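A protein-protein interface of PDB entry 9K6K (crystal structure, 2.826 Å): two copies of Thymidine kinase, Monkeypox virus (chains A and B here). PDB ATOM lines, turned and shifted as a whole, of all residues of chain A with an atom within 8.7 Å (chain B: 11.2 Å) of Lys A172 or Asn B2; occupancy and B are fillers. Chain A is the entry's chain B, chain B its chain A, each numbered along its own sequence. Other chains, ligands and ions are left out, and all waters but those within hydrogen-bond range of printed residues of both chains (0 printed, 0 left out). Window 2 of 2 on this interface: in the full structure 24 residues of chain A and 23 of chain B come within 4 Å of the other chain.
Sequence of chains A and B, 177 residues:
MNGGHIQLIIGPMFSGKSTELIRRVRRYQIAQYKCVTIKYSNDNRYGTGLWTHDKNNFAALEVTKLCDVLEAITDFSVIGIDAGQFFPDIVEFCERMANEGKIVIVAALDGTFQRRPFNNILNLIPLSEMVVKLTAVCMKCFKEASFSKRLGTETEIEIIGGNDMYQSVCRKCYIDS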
ATOM      1  N   ARG A 115     -32.044  28.794   9.698  1.00  0.00           N
ATOM      2  CA  ARG A 115     -31.389  29.979   9.144  1.00  0.00           C
ATOM      3  C   ARG A 115     -32.361  31.144   8.973  1.00  0.00           C
ATOM      4  O   ARG A 115     -32.220  31.959   8.059  1.00  0.00           O
ATOM      5  CB  ARG A 115     -30.701  29.659   7.817  1.00  0.00           C
ATOM      6  CG  ARG A 115     -29.568  28.671   7.934  1.00  0.00           C
ATOM      7  CD  ARG A 115     -28.640  28.814   6.759  1.00  0.00           C
ATOM      8  NE  ARG A 115     -29.274  28.450   5.494  1.00  0.00           N
ATOM      9  CZ  ARG A 115     -28.810  28.816   4.306  1.00  0.00           C
ATOM     10  NH1 ARG A 115     -27.721  29.566   4.233  1.00  0.00           N
ATOM     11  NH2 ARG A 115     -29.434  28.443   3.200  1.00  0.00           N
ATOM     12  N   CYS A 138     -16.510  24.036  10.480  1.00  0.00           N
ATOM     13  CA  CYS A 138     -17.493  23.050  10.052  1.00  0.00           C
ATOM     14  C   CYS A 138     -17.103  21.665  10.550  1.00  0.00           C
ATOM     15  O   CYS A 138     -15.962  21.230  10.371  1.00  0.00           O
ATOM     16  CB  CYS A 138     -17.643  23.038   8.536  1.00  0.00           C
ATOM     17  SG  CYS A 138     -18.971  21.939   8.000  1.00  0.00           S
ATOM     18  N   LYS A 140     -18.111  18.837   9.419  1.00  0.00           N
ATOM     19  CA  LYS A 140     -18.192  17.835   8.360  1.00  0.00           C
ATOM     20  C   LYS A 140     -17.087  17.983   7.328  1.00  0.00           C
ATOM     21  O   LYS A 140     -16.424  16.994   6.990  1.00  0.00           O
ATOM     22  CB  LYS A 140     -19.567  17.887   7.673  1.00  0.00           C
ATOM     23  CG  LYS A 140     -20.708  17.384   8.543  1.00  0.00           C
ATOM     24  CD  LYS A 140     -22.026  17.461   7.798  1.00  0.00           C
ATOM     25  CE  LYS A 140     -23.174  16.925   8.635  1.00  0.00           C
ATOM     26  NZ  LYS A 140     -24.460  16.998   7.879  1.00  0.00           N
ATOM     27  N   CYS A 141     -16.877  19.197   6.808  1.00  0.00           N
ATOM     28  CA  CYS A 141     -15.845  19.467   5.816  1.00  0.00           C
ATOM     29  C   CYS A 141     -14.736  20.352   6.372  1.00  0.00           C
ATOM     30  O   CYS A 141     -13.931  20.887   5.603  1.00  0.00           O
ATOM     31  CB  CYS A 141     -16.456  20.161   4.602  1.00  0.00           C
ATOM     32  SG  CYS A 141     -16.880  21.898   4.948  1.00  0.00           S
ATOM     33  N   LYS A 143     -14.246  23.290   7.256  1.00  0.00           N
ATOM     34  CA  LYS A 143     -14.060  24.625   6.707  1.00  0.00           C
ATOM     35  C   LYS A 143     -14.719  25.638   7.639  1.00  0.00           C
ATOM     36  O   LYS A 143     -15.105  25.314   8.771  1.00  0.00           O
ATOM     37  CB  LYS A 143     -14.630  24.711   5.289  1.00  0.00           C
ATOM     38  N   GLU A 144     -14.844  26.879   7.172  1.00  0.00           N
ATOM     39  CA  GLU A 144     -15.464  27.905   8.003  1.00  0.00           C
ATOM     40  C   GLU A 144     -16.972  27.697   8.037  1.00  0.00           C
ATOM     41  O   GLU A 144     -17.628  27.646   6.989  1.00  0.00           O
ATOM     42  CB  GLU A 144     -15.112  29.298   7.496  1.00  0.00           C
ATOM     43  CG  GLU A 144     -13.712  29.749   7.882  1.00  0.00           C
ATOM     44  CD  GLU A 144     -13.477  31.222   7.619  1.00  0.00           C
ATOM     45  OE1 GLU A 144     -14.416  31.898   7.152  1.00  0.00           O
ATOM     46  OE2 GLU A 144     -12.356  31.706   7.881  1.00  0.00           O
ATOM     47  N   PHE A 147     -23.378  28.499  10.072  1.00  0.00           N
ATOM     48  CA  PHE A 147     -24.760  28.156  10.351  1.00  0.00           C
ATOM     49  C   PHE A 147     -24.796  27.051  11.393  1.00  0.00           C
ATOM     50  O   PHE A 147     -23.796  26.375  11.644  1.00  0.00           O
ATOM     51  CB  PHE A 147     -25.502  27.746   9.073  1.00  0.00           C
ATOM     52  CG  PHE A 147     -25.205  28.634   7.896  1.00  0.00           C
ATOM     53  CD1 PHE A 147     -25.690  29.932   7.852  1.00  0.00           C
ATOM     54  CD2 PHE A 147     -24.452  28.168   6.830  1.00  0.00           C
ATOM     55  CE1 PHE A 147     -25.426  30.751   6.776  1.00  0.00           C
ATOM     56  CE2 PHE A 147     -24.185  28.985   5.749  1.00  0.00           C
ATOM     57  CZ  PHE A 147     -24.673  30.280   5.723  1.00  0.00           C
ATOM     58  N   LYS A 149     -27.041  23.620  12.730  1.00  0.00           N
ATOM     59  CA  LYS A 149     -27.958  22.605  12.230  1.00  0.00           C
ATOM     60  C   LYS A 149     -28.242  21.606  13.334  1.00  0.00           C
ATOM     61  O   LYS A 149     -27.312  21.006  13.888  1.00  0.00           O
ATOM     62  CB  LYS A 149     -27.396  21.890  10.994  1.00  0.00           C
ATOM     63  CG  LYS A 149     -28.356  20.861  10.410  1.00  0.00           C
ATOM     64  CD  LYS A 149     -27.893  20.337   9.060  1.00  0.00           C
ATOM     65  CE  LYS A 149     -26.585  19.564   9.165  1.00  0.00           C
ATOM     66  NZ  LYS A 149     -26.176  18.985   7.844  1.00  0.00           N
ATOM     67  N   VAL A 169     -22.081  24.211  10.794  1.00  0.00           N
ATOM     68  CA  VAL A 169     -21.782  23.784   9.439  1.00  0.00           C
ATOM     69  C   VAL A 169     -21.693  24.991   8.512  1.00  0.00           C
ATOM     70  O   VAL A 169     -22.078  26.115   8.854  1.00  0.00           O
ATOM     71  CB  VAL A 169     -22.830  22.793   8.904  1.00  0.00           C
ATOM     72  CG1 VAL A 169     -22.695  21.453   9.588  1.00  0.00           C
ATOM     73  CG2 VAL A 169     -24.221  23.353   9.139  1.00  0.00           C
ATOM     74  N   CYS A 170     -21.198  24.715   7.305  1.00  0.00           N
ATOM     75  CA  CYS A 170     -21.077  25.695   6.243  1.00  0.00           C
ATOM     76  C   CYS A 170     -22.318  25.619   5.354  1.00  0.00           C
ATOM     77  O   CYS A 170     -23.313  24.970   5.689  1.00  0.00           O
ATOM     78  CB  CYS A 170     -19.795  25.458   5.456  1.00  0.00           C
ATOM     79  SG  CYS A 170     -19.804  23.911   4.539  1.00  0.00           S
ATOM     80  N   ARG A 171     -22.255  26.270   4.190  1.00  0.00           N
ATOM     81  CA  ARG A 171     -23.418  26.354   3.313  1.00  0.00           C
ATOM     82  C   ARG A 171     -23.708  25.021   2.638  1.00  0.00           C
ATOM     83  O   ARG A 171     -24.850  24.543   2.652  1.00  0.00           O
ATOM     84  CB  ARG A 171     -23.175  27.450   2.271  1.00  0.00           C
ATOM     85  CG  ARG A 171     -24.312  27.720   1.291  1.00  0.00           C
ATOM     86  CD  ARG A 171     -23.969  28.904   0.376  1.00  0.00           C
ATOM     87  NE  ARG A 171     -24.006  30.141   1.146  1.00  0.00           N
ATOM     88  CZ  ARG A 171     -25.100  30.863   1.369  1.00  0.00           C
ATOM     89  NH1 ARG A 171     -26.271  30.470   0.878  1.00  0.00           N
ATOM     90  NH2 ARG A 171     -25.027  31.967   2.109  1.00  0.00           N
ATOM     91  N   LYS A 172     -22.673  24.378   2.091  1.00  0.00           N
ATOM     92  CA  LYS A 172     -22.873  23.146   1.332  1.00  0.00           C
ATOM     93  C   LYS A 172     -23.347  22.004   2.225  1.00  0.00           C
ATOM     94  O   LYS A 172     -24.220  21.221   1.829  1.00  0.00           O
ATOM     95  CB  LYS A 172     -21.581  22.777   0.601  1.00  0.00           C
ATOM     96  CG  LYS A 172     -21.695  21.567  -0.302  1.00  0.00           C
ATOM     97  CD  LYS A 172     -20.346  21.174  -0.890  1.00  0.00           C
ATOM     98  CE  LYS A 172     -19.328  20.857   0.201  1.00  0.00           C
ATOM     99  NZ  LYS A 172     -17.999  20.481  -0.367  1.00  0.00           N
ATOM    100  N   CYS A 173     -22.801  21.904   3.440  1.00  0.00           N
ATOM    101  CA  CYS A 173     -23.152  20.820   4.351  1.00  0.00           C
ATOM    102  C   CYS A 173     -24.489  21.031   5.044  1.00  0.00           C
ATOM    103  O   CYS A 173     -25.037  20.075   5.600  1.00  0.00           O
ATOM    104  CB  CYS A 173     -22.063  20.646   5.410  1.00  0.00           C
ATOM    105  SG  CYS A 173     -20.465  20.060   4.797  1.00  0.00           S
ATOM    106  N   TYR A 174     -25.042  22.241   5.000  1.00  0.00           N
ATOM    107  CA  TYR A 174     -26.328  22.497   5.638  1.00  0.00           C
ATOM    108  C   TYR A 174     -27.490  21.923   4.837  1.00  0.00           C
ATOM    109  O   TYR A 174     -28.528  21.589   5.416  1.00  0.00           O
ATOM    110  CB  TYR A 174     -26.511  24.006   5.841  1.00  0.00           C
ATOM    111  CG  TYR A 174     -27.817  24.393   6.496  1.00  0.00           C
ATOM    112  CD1 TYR A 174     -27.951  24.430   7.875  1.00  0.00           C
ATOM    113  CD2 TYR A 174     -28.917  24.728   5.726  1.00  0.00           C
ATOM    114  CE1 TYR A 174     -29.153  24.786   8.463  1.00  0.00           C
ATOM    115  CE2 TYR A 174     -30.115  25.076   6.302  1.00  0.00           C
ATOM    116  CZ  TYR A 174     -30.232  25.107   7.666  1.00  0.00           C
ATOM    117  OH  TYR A 174     -31.438  25.464   8.224  1.00  0.00           O
ATOM    118  N   ILE A 175     -27.340  21.792   3.522  1.00  0.00           N
ATOM    119  CA  ILE A 175     -28.372  21.242   2.656  1.00  0.00           C
ATOM    120  C   ILE A 175     -27.845  19.962   2.027  1.00  0.00           C
ATOM    121  O   ILE A 175     -26.669  19.879   1.659  1.00  0.00           O
ATOM    122  CB  ILE A 175     -28.795  22.253   1.572  1.00  0.00           C
ATOM    123  CG1 ILE A 175     -27.561  22.883   0.936  1.00  0.00           C
ATOM    124  CG2 ILE A 175     -29.683  23.337   2.166  1.00  0.00           C
ATOM    125  CD1 ILE A 175     -27.892  23.870  -0.156  1.00  0.00           C
ATOM    126  N   ASP A 176     -28.714  18.964   1.908  1.00  0.00           N
ATOM    127  CA  ASP A 176     -28.311  17.670   1.364  1.00  0.00           C
ATOM    128  C   ASP A 176     -29.049  17.354   0.063  1.00  0.00           C
ATOM    129  O   ASP A 176     -28.628  16.493  -0.710  1.00  0.00           O
ATOM    130  CB  ASP A 176     -28.558  16.563   2.390  1.00  0.00           C
ATOM    131  CG  ASP A 176     -28.002  16.904   3.759  1.00  0.00           C
ATOM    132  OD1 ASP A 176     -26.799  16.660   3.993  1.00  0.00           O
ATOM    133  OD2 ASP A 176     -28.769  17.417   4.601  1.00  0.00           O
ATOM    134  N   ASN B   2     -24.720  26.640  -1.894  1.00  0.00           N
ATOM    135  CA  ASN B   2     -23.979  25.451  -2.290  1.00  0.00           C
ATOM    136  C   ASN B   2     -22.486  25.667  -2.076  1.00  0.00           C
ATOM    137  O   ASN B   2     -21.957  25.393  -1.002  1.00  0.00           O
ATOM    138  CB  ASN B   2     -24.266  25.103  -3.749  1.00  0.00           C
ATOM    139  CG  ASN B   2     -24.083  23.627  -4.048  1.00  0.00           C
ATOM    140  OD1 ASN B   2     -24.268  22.781  -3.170  1.00  0.00           O
ATOM    141  ND2 ASN B   2     -23.726  23.309  -5.301  1.00  0.00           N
ATOM    142  N   GLY B   3     -21.808  26.176  -3.100  1.00  0.00           N
ATOM    143  CA  GLY B   3     -20.376  26.364  -3.016  1.00  0.00           C
ATOM    144  C   GLY B   3     -19.986  27.801  -2.754  1.00  0.00           C
ATOM    145  O   GLY B   3     -18.835  28.086  -2.412  1.00  0.00           O
ATOM    146  N   GLY B   4     -20.934  28.722  -2.907  1.00  0.00           N
ATOM    147  CA  GLY B   4     -20.659  30.131  -2.742  1.00  0.00           C
ATOM    148  C   GLY B   4     -20.832  30.587  -1.305  1.00  0.00           C
ATOM    149  O   GLY B   4     -20.924  29.791  -0.368  1.00  0.00           O
ATOM    150  N   HIS B   5     -20.863  31.907  -1.141  1.00  0.00           N
ATOM    151  CA  HIS B   5     -21.093  32.505   0.165  1.00  0.00           C
ATOM    152  C   HIS B   5     -21.544  33.945  -0.026  1.00  0.00           C
ATOM    153  O   HIS B   5     -21.632  34.447  -1.152  1.00  0.00           O
ATOM    154  CB  HIS B   5     -19.857  32.413   1.060  1.00  0.00           C
ATOM    155  CG  HIS B   5     -18.692  33.222   0.589  1.00  0.00           C
ATOM    156  ND1 HIS B   5     -17.728  32.717  -0.253  1.00  0.00           N
ATOM    157  CD2 HIS B   5     -18.331  34.499   0.856  1.00  0.00           C
ATOM    158  CE1 HIS B   5     -16.817  33.646  -0.480  1.00  0.00           C
ATOM    159  NE2 HIS B   5     -17.159  34.737   0.180  1.00  0.00           N
ATOM    160  N   ILE B   6     -21.872  34.588   1.092  1.00  0.00           N
ATOM    161  CA  ILE B   6     -22.373  35.954   1.122  1.00  0.00           C
ATOM    162  C   ILE B   6     -21.572  36.765   2.130  1.00  0.00           C
ATOM    163  O   ILE B   6     -21.471  36.395   3.311  1.00  0.00           O
ATOM    164  CB  ILE B   6     -23.871  36.015   1.467  1.00  0.00           C
ATOM    165  CG1 ILE B   6     -24.689  35.239   0.429  1.00  0.00           C
ATOM    166  CG2 ILE B   6     -24.324  37.466   1.575  1.00  0.00           C
ATOM    167  CD1 ILE B   6     -26.161  35.180   0.746  1.00  0.00           C
ATOM    168  N   PHE B  93     -32.460  36.745  -4.119  1.00  0.00           N
ATOM    169  CA  PHE B  93     -31.402  36.821  -5.114  1.00  0.00           C
ATOM    170  C   PHE B  93     -30.103  36.244  -4.571  1.00  0.00           C
ATOM    171  O   PHE B  93     -29.576  35.257  -5.103  1.00  0.00           O
ATOM    172  CB  PHE B  93     -31.198  38.273  -5.555  1.00  0.00           C
ATOM    173  CG  PHE B  93     -30.068  38.452  -6.526  1.00  0.00           C
ATOM    174  CD1 PHE B  93     -30.257  38.233  -7.886  1.00  0.00           C
ATOM    175  CD2 PHE B  93     -28.807  38.811  -6.074  1.00  0.00           C
ATOM    176  CE1 PHE B  93     -29.205  38.389  -8.783  1.00  0.00           C
ATOM    177  CE2 PHE B  93     -27.755  38.962  -6.952  1.00  0.00           C
ATOM    178  CZ  PHE B  93     -27.952  38.755  -8.315  1.00  0.00           C
ATOM    179  N   CYS B  94     -29.618  36.784  -3.449  1.00  0.00           N
ATOM    180  CA  CYS B  94     -28.279  36.414  -2.997  1.00  0.00           C
ATOM    181  C   CYS B  94     -28.198  34.933  -2.679  1.00  0.00           C
ATOM    182  O   CYS B  94     -27.261  34.245  -3.109  1.00  0.00           O
ATOM    183  CB  CYS B  94     -27.885  37.239  -1.779  1.00  0.00           C
ATOM    184  SG  CYS B  94     -27.720  38.989  -2.101  1.00  0.00           S
ATOM    185  N   GLU B  95     -29.243  34.401  -2.051  1.00  0.00           N
ATOM    186  CA  GLU B  95     -29.249  32.988  -1.719  1.00  0.00           C
ATOM    187  C   GLU B  95     -29.149  32.165  -2.991  1.00  0.00           C
ATOM    188  O   GLU B  95     -28.249  31.325  -3.132  1.00  0.00           O
ATOM    189  CB  GLU B  95     -30.527  32.659  -0.941  1.00  0.00           C
ATOM    190  CG  GLU B  95     -30.656  31.227  -0.444  1.00  0.00           C
ATOM    191  CD  GLU B  95     -29.829  30.952   0.794  1.00  0.00           C
ATOM    192  OE1 GLU B  95     -30.167  29.997   1.525  1.00  0.00           O
ATOM    193  OE2 GLU B  95     -28.856  31.695   1.049  1.00  0.00           O
ATOM    194  N   ARG B  96     -29.990  32.473  -3.977  1.00  0.00           N
ATOM    195  CA  ARG B  96     -29.912  31.745  -5.235  1.00  0.00           C
ATOM    196  C   ARG B  96     -28.502  31.828  -5.806  1.00  0.00           C
ATOM    197  O   ARG B  96     -27.893  30.804  -6.140  1.00  0.00           O
ATOM    198  CB  ARG B  96     -30.948  32.287  -6.217  1.00  0.00           C
ATOM    199  CG  ARG B  96     -30.972  31.582  -7.551  1.00  0.00           C
ATOM    200  CD  ARG B  96     -31.396  30.131  -7.432  1.00  0.00           C
ATOM    201  NE  ARG B  96     -31.499  29.522  -8.758  1.00  0.00           N
ATOM    202  CZ  ARG B  96     -31.922  28.284  -8.986  1.00  0.00           C
ATOM    203  NH1 ARG B  96     -32.290  27.506  -7.976  1.00  0.00           N
ATOM    204  NH2 ARG B  96     -31.981  27.829 -10.227  1.00  0.00           N
ATOM    205  N   MET B  97     -27.927  33.033  -5.832  1.00  0.00           N
ATOM    206  CA  MET B  97     -26.597  33.154  -6.412  1.00  0.00           C
ATOM    207  C   MET B  97     -25.575  32.394  -5.577  1.00  0.00           C
ATOM    208  O   MET B  97     -24.738  31.661  -6.125  1.00  0.00           O
ATOM    209  CB  MET B  97     -26.208  34.628  -6.553  1.00  0.00           C
ATOM    210  CG  MET B  97     -27.206  35.514  -7.310  1.00  0.00           C
ATOM    211  SD  MET B  97     -27.874  34.840  -8.851  1.00  0.00           S
ATOM    212  CE  MET B  97     -26.411  34.612  -9.848  1.00  0.00           C
ATOM    213  N   ALA B  98     -25.693  32.471  -4.240  1.00  0.00           N
ATOM    214  CA  ALA B  98     -24.750  31.750  -3.392  1.00  0.00           C
ATOM    215  C   ALA B  98     -24.923  30.247  -3.535  1.00  0.00           C
ATOM    216  O   ALA B  98     -23.962  29.492  -3.343  1.00  0.00           O
ATOM    217  CB  ALA B  98     -24.918  32.163  -1.933  1.00  0.00           C
ATOM    218  N   ASN B  99     -26.128  29.796  -3.887  1.00  0.00           N
ATOM    219  CA  ASN B  99     -26.356  28.373  -4.095  1.00  0.00           C
ATOM    220  C   ASN B  99     -25.927  27.897  -5.474  1.00  0.00           C
ATOM    221  O   ASN B  99     -25.992  26.693  -5.739  1.00  0.00           O
ATOM    222  CB  ASN B  99     -27.828  28.033  -3.851  1.00  0.00           C
ATOM    223  CG  ASN B  99     -28.206  28.119  -2.383  1.00  0.00           C
ATOM    224  OD1 ASN B  99     -27.411  28.556  -1.553  1.00  0.00           O
ATOM    225  ND2 ASN B  99     -29.418  27.696  -2.056  1.00  0.00           N
ATOM    226  N   GLU B 100     -25.497  28.800  -6.357  1.00  0.00           N
ATOM    227  CA  GLU B 100     -24.973  28.411  -7.661  1.00  0.00           C
ATOM    228  C   GLU B 100     -23.452  28.422  -7.693  1.00  0.00           C
ATOM    229  O   GLU B 100     -22.861  28.383  -8.780  1.00  0.00           O
ATOM    230  CB  GLU B 100     -25.534  29.324  -8.748  1.00  0.00           C
ATOM    231  CG  GLU B 100     -27.043  29.259  -8.859  1.00  0.00           C
ATOM    232  CD  GLU B 100     -27.578  30.107  -9.991  1.00  0.00           C
ATOM    233  OE1 GLU B 100     -26.799  30.412 -10.919  1.00  0.00           O
ATOM    234  OE2 GLU B 100     -28.775  30.467  -9.954  1.00  0.00           O
ATOM    235  N   GLY B 101     -22.815  28.468  -6.523  1.00  0.00           N
ATOM    236  CA  GLY B 101     -21.377  28.555  -6.398  1.00  0.00           C
ATOM    237  C   GLY B 101     -20.801  29.946  -6.491  1.00  0.00           C
ATOM    238  O   GLY B 101     -19.574  30.084  -6.520  1.00  0.00           O
ATOM    239  N   LYS B 102     -21.631  30.983  -6.478  1.00  0.00           N
ATOM    240  CA  LYS B 102     -21.162  32.346  -6.686  1.00  0.00           C
ATOM    241  C   LYS B 102     -20.936  33.084  -5.369  1.00  0.00           C
ATOM    242  O   LYS B 102     -21.629  32.860  -4.376  1.00  0.00           O
ATOM    243  CB  LYS B 102     -22.142  33.131  -7.558  1.00  0.00           C
ATOM    244  CG  LYS B 102     -22.377  32.500  -8.925  1.00  0.00           C
ATOM    245  CD  LYS B 102     -23.256  33.365  -9.794  1.00  0.00           C
ATOM    246  CE  LYS B 102     -23.598  32.669 -11.097  1.00  0.00           C
ATOM    247  NZ  LYS B 102     -22.378  32.157 -11.770  1.00  0.00           N
ATOM    248  N   ILE B 103     -19.931  33.953  -5.373  1.00  0.00           N
ATOM    249  CA  ILE B 103     -19.586  34.783  -4.227  1.00  0.00           C
ATOM    250  C   ILE B 103     -20.383  36.075  -4.336  1.00  0.00           C
ATOM    251  O   ILE B 103     -20.313  36.767  -5.359  1.00  0.00           O
ATOM    252  CB  ILE B 103     -18.081  35.073  -4.201  1.00  0.00           C
ATOM    253  CG1 ILE B 103     -17.300  33.777  -4.005  1.00  0.00           C
ATOM    254  CG2 ILE B 103     -17.749  36.061  -3.088  1.00  0.00           C
ATOM    255  CD1 ILE B 103     -15.821  33.934  -4.292  1.00  0.00           C
ATOM    256  N   VAL B 104     -21.148  36.398  -3.295  1.00  0.00           N
ATOM    257  CA  VAL B 104     -22.016  37.573  -3.294  1.00  0.00           C
ATOM    258  C   VAL B 104     -21.525  38.553  -2.233  1.00  0.00           C
ATOM    259  O   VAL B 104     -21.408  38.197  -1.060  1.00  0.00           O
ATOM    260  CB  VAL B 104     -23.483  37.183  -3.065  1.00  0.00           C
ATOM    261  CG1 VAL B 104     -24.370  38.411  -3.109  1.00  0.00           C
ATOM    262  CG2 VAL B 104     -23.916  36.186  -4.118  1.00  0.00           C
ATOM    263  N   LEU B 127     -28.388  34.384   6.720  1.00  0.00           N
ATOM    264  CA  LEU B 127     -27.979  33.610   5.558  1.00  0.00           C
ATOM    265  C   LEU B 127     -26.566  33.930   5.105  1.00  0.00           C
ATOM    266  O   LEU B 127     -26.038  33.227   4.234  1.00  0.00           O
ATOM    267  CB  LEU B 127     -28.948  33.844   4.382  1.00  0.00           C
ATOM    268  CG  LEU B 127     -30.352  33.224   4.427  1.00  0.00           C
ATOM    269  CD1 LEU B 127     -31.215  33.827   5.530  1.00  0.00           C
ATOM    270  CD2 LEU B 127     -31.051  33.395   3.110  1.00  0.00           C
ATOM    271  N   SER B 128     -25.940  34.957   5.672  1.00  0.00           N
ATOM    272  CA  SER B 128     -24.637  35.409   5.211  1.00  0.00           C
ATOM    273  C   SER B 128     -23.512  34.719   5.966  1.00  0.00           C
ATOM    274  O   SER B 128     -23.633  34.389   7.150  1.00  0.00           O
ATOM    275  CB  SER B 128     -24.505  36.925   5.358  1.00  0.00           C
ATOM    276  OG  SER B 128     -25.576  37.588   4.715  1.00  0.00           O
ATOM    277  N   GLU B 129     -22.398  34.519   5.264  1.00  0.00           N
ATOM    278  CA  GLU B 129     -21.206  33.957   5.875  1.00  0.00           C
ATOM    279  C   GLU B 129     -20.358  35.009   6.574  1.00  0.00           C
ATOM    280  O   GLU B 129     -19.701  34.692   7.570  1.00  0.00           O
ATOM    281  CB  GLU B 129     -20.367  33.230   4.824  1.00  0.00           C
ATOM    282  CG  GLU B 129     -20.816  31.797   4.525  1.00  0.00           C
ATOM    283  CD  GLU B 129     -21.966  31.693   3.522  1.00  0.00           C
ATOM    284  OE1 GLU B 129     -22.618  32.715   3.222  1.00  0.00           O
ATOM    285  OE2 GLU B 129     -22.202  30.573   3.021  1.00  0.00           O
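The backbone carbonyl oxygen of Asn B2 lies close to the backbone NH of Lys A172, at 3.3 Å. The guanidinium group (NE) of Arg A171 sits close to the backbone carbonyl oxygen (O) of Gly B4, at 3.5 Å. The guanidinium group (NH1) of Arg A115 is in salt-bridge range of the side-chain carboxylate (OE1) of Glu B95 (3.7 Å). The side-chain carboxylate of Glu B95 is in salt-bridge range of the guanidinium group of Arg A171, 2.9 Å away. OD1 of Asn B99 lies within hydrogen-bond range of NH1 of Arg A171. NH2 of Arg A171 sits at hydrogen-bond distance from O of Leu B127 (2.7 Å). The side-chain carboxylate (OE2) of Glu B129 is in salt-bridge range of the guanidinium group (NE) of Arg A171 (2.6 Å).
The side-chain amide oxygen (OD1) of Asn B99 sits close to the backbone NH (N) of Asn B2, at 3.3 Å. O of Ala B98 lies within hydrogen-bond range of N of Gly B4 (3.2 Å). The backbone NH of His B5 sits at hydrogen-bond distance from the backbone carbonyl oxygen of Lys B102, at 3.5 Å. N of Val B104 is in hydrogen-bond range of O of His B5 (2.9 Å). The backbone carbonyl oxygen (O) of Ile B6 sits at hydrogen-bond distance from the backbone NH (N) of Glu B129 (2.9 Å). The backbone carbonyl oxygen (O) of Glu B95 lies close to the side-chain amide oxygen (OD1) of Asn B99 (3.3 Å).
Arg A115 touches Leu B127. Phe A147 touches Leu B127. Glu B129 touches Phe A147. Asn B2 touches Arg A171 (N to CD, 3.3 Å). Arg A171 touches His B5. Ile B6 touches Arg A171 (CD1 to NH2, 3.7 Å). Ala B98 touches Arg A171.
Lys A172 touches just one residue of chain B: Asn B2 (3.1 Å). Of chain A, only Arg A171 (3.3 Å) and Lys A172 (3.1 Å) come within 4 Å of Asn B2. No residue of chain B comes within 4 Å of Cys A170. Printed residues of chain B within 4 Å of Arg A171: Asn B2 (3.3 Å), Gly B4 (3.3 Å), His B5 (3.9 Å), Ile B6 (3.7 Å), Glu B95 (2.9 Å), Ala B98 (3.5 Å), Asn B99 (3.3 Å), Leu B127 (2.7 Å) and Glu B129 (2.6 Å). No residue of chain B comes within 4 Å of Ile A175. No residue of chain B comes within 4 Å of Asp A176. No residue of chain A comes within 4 Å of Gly B3. Printed residues of chain A within 4 Å of Gly B4: Arg A171. Printed residues of chain A within 4 Å of Ile B6: Arg A171 (3.7 Å). Of the printed residues of chain A, Asn B99 touches Arg A171 (3.3 Å). The nearest residue of chain A that does not touch Asn B2 is Ile A175 (4.6 Å).
Printed residues of chain A that touch a printed residue of chain B: Arg A115, Phe A147, Arg A171 and Lys A172. Along chain A the printed residues that touch a printed residue of chain B span positions 115 to 172. Of the 20 printed residues of chain B, 9 touch a printed residue of chain A. Printed residues of chain B that touch a printed residue of chain A: Asn B2, Gly B4, His B5, Ile B6, Glu B95, Ala B98, Asn B99, Leu B127 and Glu B129.
No position is printed for both chains.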
